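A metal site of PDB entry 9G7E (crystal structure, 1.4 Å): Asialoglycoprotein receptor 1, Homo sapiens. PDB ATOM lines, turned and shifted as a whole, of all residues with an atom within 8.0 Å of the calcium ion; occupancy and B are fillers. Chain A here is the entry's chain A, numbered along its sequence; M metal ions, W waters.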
ATOM      1  N   HIS A  15      38.089 -28.253   6.323  1.00  0.00           N
ATOM      2  CA  HIS A  15      38.186 -28.088   4.872  1.00  0.00           C
ATOM      3  C   HIS A  15      37.804 -26.678   4.458  1.00  0.00           C
ATOM      4  O   HIS A  15      36.652 -26.272   4.675  1.00  0.00           O
ATOM      5  CB  HIS A  15      37.292 -29.098   4.144  1.00  0.00           C
ATOM      6  CG  HIS A  15      37.293 -28.952   2.645  1.00  0.00           C
ATOM      7  ND1 HIS A  15      38.237 -29.567   1.858  1.00  0.00           N
ATOM      8  CD2 HIS A  15      36.446 -28.259   1.854  1.00  0.00           C
ATOM      9  CE1 HIS A  15      37.946 -29.248   0.615  1.00  0.00           C
ATOM     10  NE2 HIS A  15      36.872 -28.458   0.555  1.00  0.00           N
ATOM     11  N   GLU A  16      38.756 -25.956   3.845  1.00  0.00           N
ATOM     12  CA  GLU A  16      38.550 -24.596   3.336  1.00  0.00           C
ATOM     13  C   GLU A  16      37.768 -23.659   4.281  1.00  0.00           C
ATOM     14  O   GLU A  16      36.683 -23.180   3.922  1.00  0.00           O
ATOM     15  CB  GLU A  16      37.888 -24.630   1.940  1.00  0.00           C
ATOM     16  CG  GLU A  16      38.701 -25.390   0.900  1.00  0.00           C
ATOM     17  CD  GLU A  16      39.744 -24.557   0.165  1.00  0.00           C
ATOM     18  OE1 GLU A  16      40.395 -23.706   0.816  1.00  0.00           O
ATOM     19  OE2 GLU A  16      39.921 -24.774  -1.059  1.00  0.00           O
ATOM     20  N   ARG A  17      38.286 -23.437   5.497  1.00  0.00           N
ATOM     21  CA  ARG A  17      37.694 -22.525   6.504  1.00  0.00           C
ATOM     22  C   ARG A  17      36.375 -23.046   7.119  1.00  0.00           C
ATOM     23  O   ARG A  17      35.650 -22.289   7.769  1.00  0.00           O
ATOM     24  CB  ARG A  17      37.527 -21.101   5.915  1.00  0.00           C
ATOM     25  CG  ARG A  17      37.313 -19.983   6.951  1.00  0.00           C
ATOM     26  CD  ARG A  17      37.277 -18.610   6.316  1.00  0.00           C
ATOM     27  NE  ARG A  17      36.657 -17.603   7.183  1.00  0.00           N
ATOM     28  CZ  ARG A  17      37.322 -16.852   8.059  1.00  0.00           C
ATOM     29  NH1 ARG A  17      38.633 -17.010   8.217  1.00  0.00           N
ATOM     30  NH2 ARG A  17      36.681 -15.971   8.807  1.00  0.00           N
ATOM     31  N   SER A  18      36.064 -24.335   6.939  1.00  0.00           N
ATOM     32  CA  SER A  18      34.861 -24.931   7.532  1.00  0.00           C
ATOM     33  C   SER A  18      35.190 -26.225   8.271  1.00  0.00           C
ATOM     34  O   SER A  18      36.150 -26.924   7.930  1.00  0.00           O
ATOM     35  CB  SER A  18      33.807 -25.200   6.461  1.00  0.00           C
ATOM     36  OG  SER A  18      32.818 -24.186   6.375  1.00  0.00           O
ATOM     37  N   CYS A  19      34.403 -26.537   9.278  1.00  0.00           N
ATOM     38  CA  CYS A  19      34.490 -27.753  10.067  1.00  0.00           C
ATOM     39  C   CYS A  19      33.259 -28.575   9.757  1.00  0.00           C
ATOM     40  O   CYS A  19      32.166 -28.031   9.742  1.00  0.00           O
ATOM     41  CB  CYS A  19      34.554 -27.413  11.548  1.00  0.00           C
ATOM     42  SG  CYS A  19      35.935 -26.330  11.969  1.00  0.00           S
ATOM     43  N   TYR A  20      33.445 -29.878   9.498  1.00  0.00           N
ATOM     44  CA  TYR A  20      32.349 -30.765   9.140  1.00  0.00           C
ATOM     45  C   TYR A  20      32.297 -31.955  10.049  1.00  0.00           C
ATOM     46  O   TYR A  20      33.318 -32.512  10.443  1.00  0.00           O
ATOM     47  CB  TYR A  20      32.490 -31.255   7.695  1.00  0.00           C
ATOM     48  CG  TYR A  20      32.587 -30.163   6.666  1.00  0.00           C
ATOM     49  CD1 TYR A  20      33.784 -29.479   6.451  1.00  0.00           C
ATOM     50  CD2 TYR A  20      31.493 -29.820   5.883  1.00  0.00           C
ATOM     51  CE1 TYR A  20      33.883 -28.481   5.482  1.00  0.00           C
ATOM     52  CE2 TYR A  20      31.564 -28.804   4.932  1.00  0.00           C
ATOM     53  CZ  TYR A  20      32.771 -28.154   4.717  1.00  0.00           C
ATOM     54  OH  TYR A  20      32.857 -27.156   3.771  1.00  0.00           O
ATOM     55  N   HIS A  42      25.301 -25.887  11.496  1.00  0.00           N
ATOM     56  CA  HIS A  42      24.110 -26.022  10.682  1.00  0.00           C
ATOM     57  C   HIS A  42      24.268 -27.230   9.786  1.00  0.00           C
ATOM     58  O   HIS A  42      25.387 -27.649   9.509  1.00  0.00           O
ATOM     59  CB  HIS A  42      23.874 -24.746   9.867  1.00  0.00           C
ATOM     60  CG  HIS A  42      25.051 -24.343   9.041  1.00  0.00           C
ATOM     61  ND1 HIS A  42      25.286 -24.884   7.795  1.00  0.00           N
ATOM     62  CD2 HIS A  42      26.085 -23.526   9.356  1.00  0.00           C
ATOM     63  CE1 HIS A  42      26.413 -24.350   7.369  1.00  0.00           C
ATOM     64  NE2 HIS A  42      26.947 -23.548   8.290  1.00  0.00           N
ATOM     65  N   LEU A  43      23.156 -27.740   9.207  1.00  0.00           N
ATOM     66  CA  LEU A  43      23.220 -28.814   8.215  1.00  0.00           C
ATOM     67  C   LEU A  43      24.048 -28.268   7.032  1.00  0.00           C
ATOM     68  O   LEU A  43      23.922 -27.084   6.690  1.00  0.00           O
ATOM     69  CB  LEU A  43      21.806 -29.158   7.760  1.00  0.00           C
ATOM     70  CG  LEU A  43      21.079 -30.183   8.596  1.00  0.00           C
ATOM     71  CD1 LEU A  43      19.597 -30.255   8.181  1.00  0.00           C
ATOM     72  CD2 LEU A  43      21.781 -31.550   8.502  1.00  0.00           C
ATOM     73  N   VAL A  44      24.967 -29.072   6.481  1.00  0.00           N
ATOM     74  CA  VAL A  44      25.926 -28.593   5.481  1.00  0.00           C
ATOM     75  C   VAL A  44      25.305 -27.741   4.363  1.00  0.00           C
ATOM     76  O   VAL A  44      24.247 -28.082   3.833  1.00  0.00           O
ATOM     77  CB  VAL A  44      26.761 -29.768   4.906  1.00  0.00           C
ATOM     78  CG1 VAL A  44      25.888 -30.719   4.097  1.00  0.00           C
ATOM     79  CG2 VAL A  44      27.946 -29.285   4.103  1.00  0.00           C
ATOM     80  N   VAL A  45      25.946 -26.600   4.062  1.00  0.00           N
ATOM     81  CA  VAL A  45      25.524 -25.688   3.000  1.00  0.00           C
ATOM     82  C   VAL A  45      26.572 -25.775   1.887  1.00  0.00           C
ATOM     83  O   VAL A  45      27.709 -25.345   2.075  1.00  0.00           O
ATOM     84  CB  VAL A  45      25.338 -24.253   3.501  1.00  0.00           C
ATOM     85  CG1 VAL A  45      25.045 -23.298   2.334  1.00  0.00           C
ATOM     86  CG2 VAL A  45      24.229 -24.192   4.544  1.00  0.00           C
ATOM     87  N   VAL A  46      26.204 -26.335   0.742  1.00  0.00           N
ATOM     88  CA  VAL A  46      27.148 -26.580  -0.331  1.00  0.00           C
ATOM     89  C   VAL A  46      27.130 -25.450  -1.339  1.00  0.00           C
ATOM     90  O   VAL A  46      26.128 -25.311  -2.054  1.00  0.00           O
ATOM     91  CB  VAL A  46      26.842 -27.926  -1.006  1.00  0.00           C
ATOM     92  CG1 VAL A  46      27.921 -28.260  -2.038  1.00  0.00           C
ATOM     93  CG2 VAL A  46      26.702 -29.053   0.023  1.00  0.00           C
ATOM     94  N   THR A  47      28.240 -24.665  -1.434  1.00  0.00           N
ATOM     95  CA  THR A  47      28.313 -23.512  -2.350  1.00  0.00           C
ATOM     96  C   THR A  47      29.350 -23.596  -3.455  1.00  0.00           C
ATOM     97  O   THR A  47      29.552 -22.587  -4.139  1.00  0.00           O
ATOM     98  CB  THR A  47      28.526 -22.227  -1.573  1.00  0.00           C
ATOM     99  OG1 THR A  47      29.731 -22.357  -0.840  1.00  0.00           O
ATOM    100  CG2 THR A  47      27.343 -21.869  -0.666  1.00  0.00           C
ATOM    101  N   SER A  48      30.015 -24.733  -3.634  1.00  0.00           N
ATOM    102  CA  SER A  48      30.976 -24.887  -4.724  1.00  0.00           C
ATOM    103  C   SER A  48      31.109 -26.336  -5.157  1.00  0.00           C
ATOM    104  O   SER A  48      30.704 -27.261  -4.429  1.00  0.00           O
ATOM    105  CB  SER A  48      32.350 -24.341  -4.324  1.00  0.00           C
ATOM    106  OG  SER A  48      32.989 -25.184  -3.377  1.00  0.00           O
ATOM    107  N   GLU A  51      33.483 -28.012  -2.705  1.00  0.00           N
ATOM    108  CA  GLU A  51      32.865 -28.430  -1.444  1.00  0.00           C
ATOM    109  C   GLU A  51      32.013 -29.680  -1.621  1.00  0.00           C
ATOM    110  O   GLU A  51      32.041 -30.578  -0.783  1.00  0.00           O
ATOM    111  CB  GLU A  51      32.056 -27.288  -0.819  1.00  0.00           C
ATOM    112  CG  GLU A  51      31.455 -27.635   0.521  1.00  0.00           C
ATOM    113  CD  GLU A  51      30.812 -26.469   1.232  1.00  0.00           C
ATOM    114  OE1 GLU A  51      30.695 -26.517   2.483  1.00  0.00           O
ATOM    115  OE2 GLU A  51      30.402 -25.501   0.550  1.00  0.00           O
ATOM    116  N   VAL A  55      32.514 -33.252   0.367  1.00  0.00           N
ATOM    117  CA  VAL A  55      31.443 -33.909   1.115  1.00  0.00           C
ATOM    118  C   VAL A  55      31.216 -35.316   0.595  1.00  0.00           C
ATOM    119  O   VAL A  55      31.177 -36.259   1.372  1.00  0.00           O
ATOM    120  CB  VAL A  55      30.141 -33.068   1.151  1.00  0.00           C
ATOM    121  CG1 VAL A  55      28.966 -33.904   1.675  1.00  0.00           C
ATOM    122  CG2 VAL A  55      30.326 -31.813   2.001  1.00  0.00           C
ATOM    123  N   TRP A  77      18.508 -22.241   1.920  1.00  0.00           N
ATOM    124  CA  TRP A  77      19.600 -22.867   2.654  1.00  0.00           C
ATOM    125  C   TRP A  77      19.428 -22.460   4.133  1.00  0.00           C
ATOM    126  O   TRP A  77      18.978 -21.338   4.433  1.00  0.00           O
ATOM    127  CB  TRP A  77      20.966 -22.419   2.097  1.00  0.00           C
ATOM    128  CG  TRP A  77      21.306 -23.015   0.755  1.00  0.00           C
ATOM    129  CD1 TRP A  77      21.268 -22.376  -0.452  1.00  0.00           C
ATOM    130  CD2 TRP A  77      21.817 -24.330   0.497  1.00  0.00           C
ATOM    131  NE1 TRP A  77      21.726 -23.218  -1.438  1.00  0.00           N
ATOM    132  CE2 TRP A  77      22.093 -24.420  -0.882  1.00  0.00           C
ATOM    133  CE3 TRP A  77      22.143 -25.438   1.309  1.00  0.00           C
ATOM    134  CZ2 TRP A  77      22.611 -25.570  -1.476  1.00  0.00           C
ATOM    135  CZ3 TRP A  77      22.676 -26.569   0.720  1.00  0.00           C
ATOM    136  CH2 TRP A  77      22.883 -26.635  -0.655  1.00  0.00           C
ATOM    137  N   ASP A  79      21.345 -21.520   6.433  1.00  0.00           N
ATOM    138  CA  ASP A  79      22.084 -20.355   6.952  1.00  0.00           C
ATOM    139  C   ASP A  79      21.778 -19.032   6.212  1.00  0.00           C
ATOM    140  O   ASP A  79      22.492 -18.041   6.400  1.00  0.00           O
ATOM    141  CB  ASP A  79      23.592 -20.633   6.980  1.00  0.00           C
ATOM    142  CG  ASP A  79      24.249 -20.714   5.613  1.00  0.00           C
ATOM    143  OD1 ASP A  79      23.505 -20.804   4.609  1.00  0.00           O
ATOM    144  OD2 ASP A  79      25.485 -20.662   5.546  1.00  0.00           O
ATOM    145  N   THR A  81      21.994 -18.545   2.921  1.00  0.00           N
ATOM    146  CA  THR A  81      22.698 -18.506   1.622  1.00  0.00           C
ATOM    147  C   THR A  81      21.645 -18.543   0.511  1.00  0.00           C
ATOM    148  O   THR A  81      20.723 -19.366   0.578  1.00  0.00           O
ATOM    149  CB  THR A  81      23.655 -19.692   1.472  1.00  0.00           C
ATOM    150  OG1 THR A  81      24.661 -19.612   2.483  1.00  0.00           O
ATOM    151  CG2 THR A  81      24.328 -19.752   0.095  1.00  0.00           C
ATOM    152  N   GLU A 132      27.989 -28.524   9.598  1.00  0.00           N
ATOM    153  CA  GLU A 132      29.040 -27.637   9.170  1.00  0.00           C
ATOM    154  C   GLU A 132      29.077 -26.420  10.069  1.00  0.00           C
ATOM    155  O   GLU A 132      28.042 -25.876  10.444  1.00  0.00           O
ATOM    156  CB  GLU A 132      28.807 -27.215   7.717  1.00  0.00           C
ATOM    157  CG  GLU A 132      29.949 -26.403   7.152  1.00  0.00           C
ATOM    158  CD  GLU A 132      29.719 -25.820   5.766  1.00  0.00           C
ATOM    159  OE1 GLU A 132      28.645 -26.085   5.172  1.00  0.00           O
ATOM    160  OE2 GLU A 132      30.597 -25.085   5.285  1.00  0.00           O
ATOM    161  N   THR A 133      30.277 -25.990  10.431  1.00  0.00           N
ATOM    162  CA  THR A 133      30.497 -24.761  11.161  1.00  0.00           C
ATOM    163  C   THR A 133      31.621 -24.001  10.455  1.00  0.00           C
ATOM    164  O   THR A 133      32.493 -24.623   9.862  1.00  0.00           O
ATOM    165  CB  THR A 133      30.654 -24.989  12.652  1.00  0.00           C
ATOM    166  OG1 THR A 133      30.278 -23.805  13.318  1.00  0.00           O
ATOM    167  CG2 THR A 133      32.041 -25.402  13.042  1.00  0.00           C
ATOM    168  N   GLU A 134      31.560 -22.673  10.424  1.00  0.00           N
ATOM    169  CA  GLU A 134      32.563 -21.888   9.723  1.00  0.00           C
ATOM    170  C   GLU A 134      33.586 -21.369  10.699  1.00  0.00           C
ATOM    171  O   GLU A 134      33.206 -20.739  11.695  1.00  0.00           O
ATOM    172  CB  GLU A 134      31.931 -20.731   8.940  1.00  0.00           C
ATOM    173  CG  GLU A 134      31.164 -21.180   7.712  1.00  0.00           C
ATOM    174  CD  GLU A 134      29.725 -21.565   7.993  1.00  0.00           C
ATOM    175  OE1 GLU A 134      29.182 -22.413   7.257  1.00  0.00           O
ATOM    176  OE2 GLU A 134      29.153 -21.021   8.962  1.00  0.00           O
HETATM  177 CA    CA M   1      29.581 -24.578   3.179  1.00  0.00          CA
HETATM  178  O   HOH W   1      29.057 -22.686   1.938  1.00  0.00           O
HETATM  179  O   HOH W   2      31.833 -23.339   2.931  1.00  0.00           O
HETATM  180  O   HOH W   3      28.798 -22.811   4.658  1.00  0.00           O
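OG of Ser 48 sits at hydrogen-bond distance from N of Glu 51 (2.9 Å).
The side-chain carboxylate (OE2) of Glu 132 sits close to the side-chain hydroxyl (OH) of Tyr 20, 3.4 Å away.
The side-chain hydroxyl (OH) of Tyr 20 sits close to the side-chain carboxylate (OE1) of Glu 51.
The backbone NH (N) of Glu 132 is in hydrogen-bond range of the backbone carbonyl oxygen (O) of His 42.
OE2 of Glu 132 sits close to OG of Ser 18 (2.6 Å).
OE2 of Glu 51 sits at hydrogen-bond distance from N of Thr 47, at 3.1 Å.
Within 4 Å of the calcium ion: Val 45, Glu 51 and Glu 132.
O of Val 45 is bound to the calcium ion.
Water W1 is bound to the calcium ion (2.3 Å).
The calcium ion is bound by the side-chain carboxylate (OE1) of Glu 51 (2.3 Å).
The calcium ion is bound by OE2 of Glu 132.
Water W3 binds the calcium ion (2.4 Å).
Water W2 binds the calcium ion (2.6 Å).
OE1 of Glu 132 is bound to the calcium ion (2.7 Å).
The calcium ion has seven donor atoms within binding distance.
Slightly farther from the calcium ion lies OE2 of Glu 51 (2.9 Å).
Water W1 bridges OG1 of Thr 47 (2.9 Å) and OE2 of Glu 51 (3.4 Å).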
